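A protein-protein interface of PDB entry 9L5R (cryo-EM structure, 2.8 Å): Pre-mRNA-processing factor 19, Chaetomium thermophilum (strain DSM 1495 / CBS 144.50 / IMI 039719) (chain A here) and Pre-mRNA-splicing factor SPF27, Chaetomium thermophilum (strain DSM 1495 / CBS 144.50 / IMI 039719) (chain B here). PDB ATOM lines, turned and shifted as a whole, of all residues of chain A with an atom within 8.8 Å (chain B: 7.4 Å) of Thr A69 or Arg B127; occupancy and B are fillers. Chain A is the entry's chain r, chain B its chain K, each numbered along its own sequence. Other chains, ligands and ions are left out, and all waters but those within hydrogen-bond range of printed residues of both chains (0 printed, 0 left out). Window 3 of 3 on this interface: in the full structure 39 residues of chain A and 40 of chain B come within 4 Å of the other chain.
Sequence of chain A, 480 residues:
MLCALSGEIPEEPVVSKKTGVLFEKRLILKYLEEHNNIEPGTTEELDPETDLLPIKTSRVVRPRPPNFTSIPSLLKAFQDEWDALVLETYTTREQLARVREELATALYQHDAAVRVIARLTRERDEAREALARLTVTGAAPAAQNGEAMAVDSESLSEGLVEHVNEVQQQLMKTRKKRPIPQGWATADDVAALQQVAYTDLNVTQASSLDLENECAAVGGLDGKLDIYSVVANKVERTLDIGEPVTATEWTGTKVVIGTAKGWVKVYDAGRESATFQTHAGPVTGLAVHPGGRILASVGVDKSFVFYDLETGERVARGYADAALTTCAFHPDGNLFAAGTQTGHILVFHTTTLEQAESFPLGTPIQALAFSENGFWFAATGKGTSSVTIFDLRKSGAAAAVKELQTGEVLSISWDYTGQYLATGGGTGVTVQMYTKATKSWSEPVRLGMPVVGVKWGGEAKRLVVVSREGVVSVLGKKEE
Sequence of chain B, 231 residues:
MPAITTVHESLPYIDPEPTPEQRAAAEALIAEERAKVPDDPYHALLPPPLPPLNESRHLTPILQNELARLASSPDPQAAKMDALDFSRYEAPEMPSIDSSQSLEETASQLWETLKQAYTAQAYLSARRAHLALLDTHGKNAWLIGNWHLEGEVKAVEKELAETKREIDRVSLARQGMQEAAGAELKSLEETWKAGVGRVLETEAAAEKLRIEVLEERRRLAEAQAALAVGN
Hydrophobic or aromatic side chains of chain B within 4 Å of the printed part of chain A: His B130, Leu B131 and Leu B134.
Of the 14 printed residues of chain A, 4 touch a printed residue of chain B.
NE of Arg A64 is in hydrogen-bond range of O of Phe A68, 2.8 Å away.
The guanidinium group (NH2) of Arg A64 lies within hydrogen-bond range of the backbone carbonyl oxygen (O) of Thr A69, 3.1 Å away.
The side-chain hydroxyl (OG) of Ser A73 sits at hydrogen-bond distance from the backbone NH (N) of Ser A70, at 3.0 Å.
The side-chain hydroxyl (OG) of Ser A73 lies within hydrogen-bond range of the backbone NH (N) of Thr A69 (3.4 Å).
Among the printed residues, merely in contact across the chains: Arg A64 with His B130 (3.9 Å), Arg A64 with Leu B134 (3.3 Å), Pro A65 with Leu B134 (3.7 Å), Thr A69 with Arg B127 (3.3 Å), Thr A69 with His B130 (3.9 Å), Thr A69 with Leu B131 (3.9 Å), Thr A69 with Leu B134 (3.7 Å) and Ser A70 with Arg B127 (3.8 Å).
Of the printed residues of chain B, Arg A64 touches His B130 and Leu B134.
Of the printed residues of chain B, Pro A65 touches Leu B134.
Thr A69 touches just these residues of chain B: Arg B127, His B130, Leu B131 and Leu B134.
Of the printed residues of chain B, Ser A70 touches Arg B127 (3.8 Å).
No residue of chain A comes within 4 Å of Ala B126.
Of the printed residues of chain A, Arg B127 touches Thr A69 and Ser A70.
Of the printed residues of chain A, His B130 touches Arg A64 (3.9 Å) and Thr A69 (3.9 Å).
The nearest residue of chain A that does not touch Arg B127 is Ile A71 (5.6 Å).
The nearest printed residue of chain A that does not touch His B130 is Ile A71 (5.7 Å).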
ATOM      1  N   ARG A  64      -7.640 -19.849 -16.775  1.00  0.00           N
ATOM      2  CA  ARG A  64      -7.185 -18.483 -17.002  1.00  0.00           C
ATOM      3  C   ARG A  64      -7.738 -17.563 -15.919  1.00  0.00           C
ATOM      4  O   ARG A  64      -8.950 -17.556 -15.677  1.00  0.00           O
ATOM      5  CB  ARG A  64      -7.635 -18.016 -18.383  1.00  0.00           C
ATOM      6  CG  ARG A  64      -6.994 -16.735 -18.874  1.00  0.00           C
ATOM      7  CD  ARG A  64      -7.552 -16.359 -20.238  1.00  0.00           C
ATOM      8  NE  ARG A  64      -6.895 -15.189 -20.806  1.00  0.00           N
ATOM      9  CZ  ARG A  64      -5.964 -15.234 -21.748  1.00  0.00           C
ATOM     10  NH1 ARG A  64      -5.560 -16.383 -22.266  1.00  0.00           N
ATOM     11  NH2 ARG A  64      -5.429 -14.098 -22.186  1.00  0.00           N
ATOM     12  N   PRO A  65      -6.894 -16.796 -15.236  1.00  0.00           N
ATOM     13  CA  PRO A  65      -7.380 -15.917 -14.168  1.00  0.00           C
ATOM     14  C   PRO A  65      -8.045 -14.676 -14.738  1.00  0.00           C
ATOM     15  O   PRO A  65      -7.842 -14.343 -15.915  1.00  0.00           O
ATOM     16  CB  PRO A  65      -6.097 -15.569 -13.396  1.00  0.00           C
ATOM     17  CG  PRO A  65      -5.026 -15.679 -14.400  1.00  0.00           C
ATOM     18  CD  PRO A  65      -5.426 -16.769 -15.349  1.00  0.00           C
ATOM     19  N   PRO A  66      -8.876 -13.988 -13.939  1.00  0.00           N
ATOM     20  CA  PRO A  66      -9.542 -12.768 -14.437  1.00  0.00           C
ATOM     21  C   PRO A  66      -8.601 -11.651 -14.853  1.00  0.00           C
ATOM     22  O   PRO A  66      -8.909 -10.908 -15.793  1.00  0.00           O
ATOM     23  CB  PRO A  66     -10.407 -12.334 -13.244  1.00  0.00           C
ATOM     24  CG  PRO A  66      -9.882 -13.100 -12.068  1.00  0.00           C
ATOM     25  CD  PRO A  66      -9.392 -14.386 -12.620  1.00  0.00           C
ATOM     26  N   ASN A  67      -7.471 -11.492 -14.165  1.00  0.00           N
ATOM     27  CA  ASN A  67      -6.569 -10.395 -14.495  1.00  0.00           C
ATOM     28  C   ASN A  67      -5.821 -10.642 -15.799  1.00  0.00           C
ATOM     29  O   ASN A  67      -5.529  -9.693 -16.535  1.00  0.00           O
ATOM     30  CB  ASN A  67      -5.597 -10.152 -13.338  1.00  0.00           C
ATOM     31  CG  ASN A  67      -4.793 -11.392 -12.960  1.00  0.00           C
ATOM     32  OD1 ASN A  67      -4.891 -12.442 -13.595  1.00  0.00           O
ATOM     33  ND2 ASN A  67      -3.989 -11.267 -11.911  1.00  0.00           N
ATOM     34  N   PHE A  68      -5.509 -11.898 -16.102  1.00  0.00           N
ATOM     35  CA  PHE A  68      -4.649 -12.227 -17.238  1.00  0.00           C
ATOM     36  C   PHE A  68      -5.467 -12.597 -18.472  1.00  0.00           C
ATOM     37  O   PHE A  68      -5.327 -13.682 -19.033  1.00  0.00           O
ATOM     38  CB  PHE A  68      -3.699 -13.354 -16.850  1.00  0.00           C
ATOM     39  CG  PHE A  68      -2.669 -12.963 -15.820  1.00  0.00           C
ATOM     40  CD1 PHE A  68      -2.421 -11.628 -15.523  1.00  0.00           C
ATOM     41  CD2 PHE A  68      -1.973 -13.936 -15.121  1.00  0.00           C
ATOM     42  CE1 PHE A  68      -1.487 -11.277 -14.566  1.00  0.00           C
ATOM     43  CE2 PHE A  68      -1.040 -13.590 -14.161  1.00  0.00           C
ATOM     44  CZ  PHE A  68      -0.797 -12.258 -13.883  1.00  0.00           C
ATOM     45  N   THR A  69      -6.338 -11.685 -18.904  1.00  0.00           N
ATOM     46  CA  THR A  69      -7.164 -11.914 -20.082  1.00  0.00           C
ATOM     47  C   THR A  69      -6.707 -11.131 -21.304  1.00  0.00           C
ATOM     48  O   THR A  69      -7.062 -11.508 -22.426  1.00  0.00           O
ATOM     49  CB  THR A  69      -8.628 -11.567 -19.785  1.00  0.00           C
ATOM     50  OG1 THR A  69      -8.728 -10.193 -19.392  1.00  0.00           O
ATOM     51  CG2 THR A  69      -9.171 -12.454 -18.681  1.00  0.00           C
ATOM     52  N   SER A  70      -5.939 -10.066 -21.119  1.00  0.00           N
ATOM     53  CA  SER A  70      -5.409  -9.287 -22.226  1.00  0.00           C
ATOM     54  C   SER A  70      -3.971  -9.698 -22.518  1.00  0.00           C
ATOM     55  O   SER A  70      -3.269 -10.247 -21.665  1.00  0.00           O
ATOM     56  CB  SER A  70      -5.475  -7.789 -21.921  1.00  0.00           C
ATOM     57  OG  SER A  70      -4.457  -7.408 -21.015  1.00  0.00           O
ATOM     58  N   ILE A  71      -3.551  -9.439 -23.761  1.00  0.00           N
ATOM     59  CA  ILE A  71      -2.159  -9.703 -24.145  1.00  0.00           C
ATOM     60  C   ILE A  71      -1.151  -8.899 -23.329  1.00  0.00           C
ATOM     61  O   ILE A  71      -0.123  -9.473 -22.939  1.00  0.00           O
ATOM     62  CB  ILE A  71      -1.991  -9.536 -25.662  1.00  0.00           C
ATOM     63  CG1 ILE A  71      -3.067 -10.330 -26.405  1.00  0.00           C
ATOM     64  CG2 ILE A  71      -0.610  -9.995 -26.111  1.00  0.00           C
ATOM     65  CD1 ILE A  71      -3.001 -11.823 -26.164  1.00  0.00           C
ATOM     66  N   PRO A  72      -1.340  -7.594 -23.047  1.00  0.00           N
ATOM     67  CA  PRO A  72      -0.398  -6.924 -22.126  1.00  0.00           C
ATOM     68  C   PRO A  72      -0.358  -7.517 -20.725  1.00  0.00           C
ATOM     69  O   PRO A  72       0.710  -7.518 -20.098  1.00  0.00           O
ATOM     70  CB  PRO A  72      -0.904  -5.477 -22.102  1.00  0.00           C
ATOM     71  CG  PRO A  72      -1.538  -5.297 -23.409  1.00  0.00           C
ATOM     72  CD  PRO A  72      -2.232  -6.591 -23.673  1.00  0.00           C
ATOM     73  N   SER A  73      -1.487  -8.013 -20.214  1.00  0.00           N
ATOM     74  CA  SER A  73      -1.481  -8.681 -18.916  1.00  0.00           C
ATOM     75  C   SER A  73      -0.663  -9.966 -18.963  1.00  0.00           C
ATOM     76  O   SER A  73       0.111 -10.252 -18.040  1.00  0.00           O
ATOM     77  CB  SER A  73      -2.913  -8.972 -18.469  1.00  0.00           C
ATOM     78  OG  SER A  73      -3.545  -9.876 -19.357  1.00  0.00           O
ATOM     79  N   LEU A  74      -0.808 -10.740 -20.043  1.00  0.00           N
ATOM     80  CA  LEU A  74       0.015 -11.932 -20.219  1.00  0.00           C
ATOM     81  C   LEU A  74       1.488 -11.578 -20.358  1.00  0.00           C
ATOM     82  O   LEU A  74       2.349 -12.309 -19.860  1.00  0.00           O
ATOM     83  CB  LEU A  74      -0.454 -12.723 -21.440  1.00  0.00           C
ATOM     84  CG  LEU A  74      -1.873 -13.294 -21.451  1.00  0.00           C
ATOM     85  CD1 LEU A  74      -2.068 -14.188 -22.666  1.00  0.00           C
ATOM     86  CD2 LEU A  74      -2.157 -14.063 -20.174  1.00  0.00           C
ATOM     87  N   LEU A  75       1.796 -10.449 -20.998  1.00  0.00           N
ATOM     88  CA  LEU A  75       3.192 -10.054 -21.161  1.00  0.00           C
ATOM     89  C   LEU A  75       3.811  -9.611 -19.838  1.00  0.00           C
ATOM     90  O   LEU A  75       4.959  -9.963 -19.536  1.00  0.00           O
ATOM     91  CB  LEU A  75       3.296  -8.952 -22.213  1.00  0.00           C
ATOM     92  CG  LEU A  75       3.097  -9.450 -23.647  1.00  0.00           C
ATOM     93  CD1 LEU A  75       3.070  -8.296 -24.636  1.00  0.00           C
ATOM     94  CD2 LEU A  75       4.171 -10.464 -24.022  1.00  0.00           C
ATOM     95  N   LYS A  76       3.078  -8.836 -19.034  1.00  0.00           N
ATOM     96  CA  LYS A  76       3.629  -8.446 -17.738  1.00  0.00           C
ATOM     97  C   LYS A  76       3.729  -9.643 -16.799  1.00  0.00           C
ATOM     98  O   LYS A  76       4.667  -9.717 -15.994  1.00  0.00           O
ATOM     99  CB  LYS A  76       2.812  -7.309 -17.114  1.00  0.00           C
ATOM    100  CG  LYS A  76       1.394  -7.645 -16.701  1.00  0.00           C
ATOM    101  CD  LYS A  76       0.768  -6.509 -15.912  1.00  0.00           C
ATOM    102  CE  LYS A  76       0.536  -5.291 -16.790  1.00  0.00           C
ATOM    103  NZ  LYS A  76      -0.507  -5.543 -17.824  1.00  0.00           N
ATOM    104  N   ALA A  77       2.811 -10.610 -16.922  1.00  0.00           N
ATOM    105  CA  ALA A  77       2.960 -11.869 -16.200  1.00  0.00           C
ATOM    106  C   ALA A  77       4.194 -12.628 -16.669  1.00  0.00           C
ATOM    107  O   ALA A  77       4.881 -13.266 -15.863  1.00  0.00           O
ATOM    108  CB  ALA A  77       1.709 -12.726 -16.379  1.00  0.00           C
ATOM    109  N   GLN B 121      -7.547  -1.446 -29.977  1.00  0.00           N
ATOM    110  CA  GLN B 121      -8.888  -1.955 -30.249  1.00  0.00           C
ATOM    111  C   GLN B 121      -8.889  -3.470 -30.393  1.00  0.00           C
ATOM    112  O   GLN B 121      -9.735  -4.160 -29.813  1.00  0.00           O
ATOM    113  CB  GLN B 121      -9.448  -1.307 -31.515  1.00  0.00           C
ATOM    114  CG  GLN B 121     -10.218  -0.043 -31.256  1.00  0.00           C
ATOM    115  CD  GLN B 121     -11.532  -0.317 -30.566  1.00  0.00           C
ATOM    116  OE1 GLN B 121     -11.902   0.373 -29.620  1.00  0.00           O
ATOM    117  NE2 GLN B 121     -12.250  -1.328 -31.039  1.00  0.00           N
ATOM    118  N   ALA B 122      -7.943  -4.002 -31.170  1.00  0.00           N
ATOM    119  CA  ALA B 122      -7.872  -5.447 -31.361  1.00  0.00           C
ATOM    120  C   ALA B 122      -7.505  -6.163 -30.065  1.00  0.00           C
ATOM    121  O   ALA B 122      -8.073  -7.221 -29.751  1.00  0.00           O
ATOM    122  CB  ALA B 122      -6.875  -5.774 -32.470  1.00  0.00           C
ATOM    123  N   TYR B 123      -6.576  -5.588 -29.291  1.00  0.00           N
ATOM    124  CA  TYR B 123      -6.210  -6.166 -28.000  1.00  0.00           C
ATOM    125  C   TYR B 123      -7.395  -6.189 -27.041  1.00  0.00           C
ATOM    126  O   TYR B 123      -7.636  -7.193 -26.361  1.00  0.00           O
ATOM    127  CB  TYR B 123      -5.053  -5.380 -27.387  1.00  0.00           C
ATOM    128  CG  TYR B 123      -3.692  -5.740 -27.933  1.00  0.00           C
ATOM    129  CD1 TYR B 123      -3.481  -6.944 -28.594  1.00  0.00           C
ATOM    130  CD2 TYR B 123      -2.616  -4.872 -27.790  1.00  0.00           C
ATOM    131  CE1 TYR B 123      -2.236  -7.275 -29.091  1.00  0.00           C
ATOM    132  CE2 TYR B 123      -1.369  -5.194 -28.287  1.00  0.00           C
ATOM    133  CZ  TYR B 123      -1.185  -6.395 -28.937  1.00  0.00           C
ATOM    134  OH  TYR B 123       0.056  -6.719 -29.433  1.00  0.00           O
ATOM    135  N   LEU B 124      -8.157  -5.097 -26.991  1.00  0.00           N
ATOM    136  CA  LEU B 124      -9.283  -5.015 -26.070  1.00  0.00           C
ATOM    137  C   LEU B 124     -10.427  -5.921 -26.512  1.00  0.00           C
ATOM    138  O   LEU B 124     -11.136  -6.485 -25.670  1.00  0.00           O
ATOM    139  CB  LEU B 124      -9.732  -3.562 -25.953  1.00  0.00           C
ATOM    140  CG  LEU B 124     -10.812  -3.175 -24.952  1.00  0.00           C
ATOM    141  CD1 LEU B 124     -10.417  -3.608 -23.557  1.00  0.00           C
ATOM    142  CD2 LEU B 124     -10.959  -1.672 -25.004  1.00  0.00           C
ATOM    143  N   SER B 125     -10.607  -6.088 -27.825  1.00  0.00           N
ATOM    144  CA  SER B 125     -11.602  -7.035 -28.324  1.00  0.00           C
ATOM    145  C   SER B 125     -11.235  -8.469 -27.961  1.00  0.00           C
ATOM    146  O   SER B 125     -12.103  -9.251 -27.549  1.00  0.00           O
ATOM    147  CB  SER B 125     -11.752  -6.888 -29.838  1.00  0.00           C
ATOM    148  OG  SER B 125     -10.724  -7.584 -30.521  1.00  0.00           O
ATOM    149  N   ALA B 126      -9.954  -8.828 -28.100  1.00  0.00           N
ATOM    150  CA  ALA B 126      -9.514 -10.162 -27.695  1.00  0.00           C
ATOM    151  C   ALA B 126      -9.671 -10.365 -26.192  1.00  0.00           C
ATOM    152  O   ALA B 126     -10.060 -11.452 -25.740  1.00  0.00           O
ATOM    153  CB  ALA B 126      -8.066 -10.390 -28.123  1.00  0.00           C
ATOM    154  N   ARG B 127      -9.376  -9.324 -25.405  1.00  0.00           N
ATOM    155  CA  ARG B 127      -9.551  -9.401 -23.957  1.00  0.00           C
ATOM    156  C   ARG B 127     -11.015  -9.605 -23.583  1.00  0.00           C
ATOM    157  O   ARG B 127     -11.329 -10.413 -22.704  1.00  0.00           O
ATOM    158  CB  ARG B 127      -9.002  -8.137 -23.294  1.00  0.00           C
ATOM    159  CG  ARG B 127      -9.320  -8.026 -21.811  1.00  0.00           C
ATOM    160  CD  ARG B 127      -9.137  -6.610 -21.293  1.00  0.00           C
ATOM    161  NE  ARG B 127      -9.787  -6.424 -20.001  1.00  0.00           N
ATOM    162  CZ  ARG B 127     -10.178  -5.251 -19.519  1.00  0.00           C
ATOM    163  NH1 ARG B 127      -9.997  -4.130 -20.197  1.00  0.00           N
ATOM    164  NH2 ARG B 127     -10.764  -5.203 -18.327  1.00  0.00           N
ATOM    165  N   ARG B 128     -11.923  -8.888 -24.251  1.00  0.00           N
ATOM    166  CA  ARG B 128     -13.349  -9.052 -23.981  1.00  0.00           C
ATOM    167  C   ARG B 128     -13.841 -10.437 -24.387  1.00  0.00           C
ATOM    168  O   ARG B 128     -14.681 -11.029 -23.697  1.00  0.00           O
ATOM    169  CB  ARG B 128     -14.149  -7.968 -24.701  1.00  0.00           C
ATOM    170  CG  ARG B 128     -14.099  -6.607 -24.026  1.00  0.00           C
ATOM    171  CD  ARG B 128     -15.076  -5.643 -24.674  1.00  0.00           C
ATOM    172  NE  ARG B 128     -14.778  -5.436 -26.086  1.00  0.00           N
ATOM    173  CZ  ARG B 128     -15.649  -4.979 -26.976  1.00  0.00           C
ATOM    174  NH1 ARG B 128     -16.889  -4.671 -26.634  1.00  0.00           N
ATOM    175  NH2 ARG B 128     -15.266  -4.829 -28.240  1.00  0.00           N
ATOM    176  N   ALA B 129     -13.333 -10.967 -25.507  1.00  0.00           N
ATOM    177  CA  ALA B 129     -13.706 -12.316 -25.926  1.00  0.00           C
ATOM    178  C   ALA B 129     -13.245 -13.361 -24.917  1.00  0.00           C
ATOM    179  O   ALA B 129     -14.005 -14.275 -24.564  1.00  0.00           O
ATOM    180  CB  ALA B 129     -13.125 -12.614 -27.308  1.00  0.00           C
ATOM    181  N   HIS B 130     -12.009 -13.231 -24.425  1.00  0.00           N
ATOM    182  CA  HIS B 130     -11.524 -14.155 -23.405  1.00  0.00           C
ATOM    183  C   HIS B 130     -12.278 -13.995 -22.092  1.00  0.00           C
ATOM    184  O   HIS B 130     -12.502 -14.983 -21.384  1.00  0.00           O
ATOM    185  CB  HIS B 130     -10.025 -13.959 -23.186  1.00  0.00           C
ATOM    186  CG  HIS B 130      -9.189 -14.372 -24.355  1.00  0.00           C
ATOM    187  ND1 HIS B 130      -8.897 -13.519 -25.398  1.00  0.00           N
ATOM    188  CD2 HIS B 130      -8.588 -15.549 -24.651  1.00  0.00           C
ATOM    189  CE1 HIS B 130      -8.149 -14.153 -26.284  1.00  0.00           C
ATOM    190  NE2 HIS B 130      -7.947 -15.384 -25.854  1.00  0.00           N
ATOM    191  N   LEU B 131     -12.681 -12.767 -21.756  1.00  0.00           N
ATOM    192  CA  LEU B 131     -13.465 -12.535 -20.548  1.00  0.00           C
ATOM    193  C   LEU B 131     -14.837 -13.194 -20.642  1.00  0.00           C
ATOM    194  O   LEU B 131     -15.312 -13.791 -19.669  1.00  0.00           O
ATOM    195  CB  LEU B 131     -13.598 -11.033 -20.308  1.00  0.00           C
ATOM    196  CG  LEU B 131     -13.750 -10.538 -18.872  1.00  0.00           C
ATOM    197  CD1 LEU B 131     -12.772 -11.243 -17.950  1.00  0.00           C
ATOM    198  CD2 LEU B 131     -13.522  -9.040 -18.839  1.00  0.00           C
ATOM    199  N   ALA B 132     -15.482 -13.104 -21.809  1.00  0.00           N
ATOM    200  CA  ALA B 132     -16.761 -13.781 -22.006  1.00  0.00           C
ATOM    201  C   ALA B 132     -16.602 -15.298 -21.962  1.00  0.00           C
ATOM    202  O   ALA B 132     -17.456 -16.003 -21.403  1.00  0.00           O
ATOM    203  CB  ALA B 132     -17.386 -13.345 -23.330  1.00  0.00           C
ATOM    204  N   LEU B 133     -15.515 -15.816 -22.547  1.00  0.00           N
ATOM    205  CA  LEU B 133     -15.248 -17.252 -22.493  1.00  0.00           C
ATOM    206  C   LEU B 133     -15.029 -17.723 -21.059  1.00  0.00           C
ATOM    207  O   LEU B 133     -15.497 -18.801 -20.673  1.00  0.00           O
ATOM    208  CB  LEU B 133     -14.037 -17.591 -23.361  1.00  0.00           C
ATOM    209  CG  LEU B 133     -14.294 -17.685 -24.865  1.00  0.00           C
ATOM    210  CD1 LEU B 133     -12.984 -17.705 -25.636  1.00  0.00           C
ATOM    211  CD2 LEU B 133     -15.120 -18.921 -25.180  1.00  0.00           C
ATOM    212  N   LEU B 134     -14.319 -16.928 -20.257  1.00  0.00           N
ATOM    213  CA  LEU B 134     -14.129 -17.265 -18.851  1.00  0.00           C
ATOM    214  C   LEU B 134     -15.426 -17.147 -18.062  1.00  0.00           C
ATOM    215  O   LEU B 134     -15.619 -17.869 -17.079  1.00  0.00           O
ATOM    216  CB  LEU B 134     -13.057 -16.367 -18.239  1.00  0.00           C
ATOM    217  CG  LEU B 134     -11.616 -16.764 -18.548  1.00  0.00           C
ATOM    218  CD1 LEU B 134     -10.651 -15.804 -17.879  1.00  0.00           C
ATOM    219  CD2 LEU B 134     -11.353 -18.197 -18.111  1.00  0.00           C
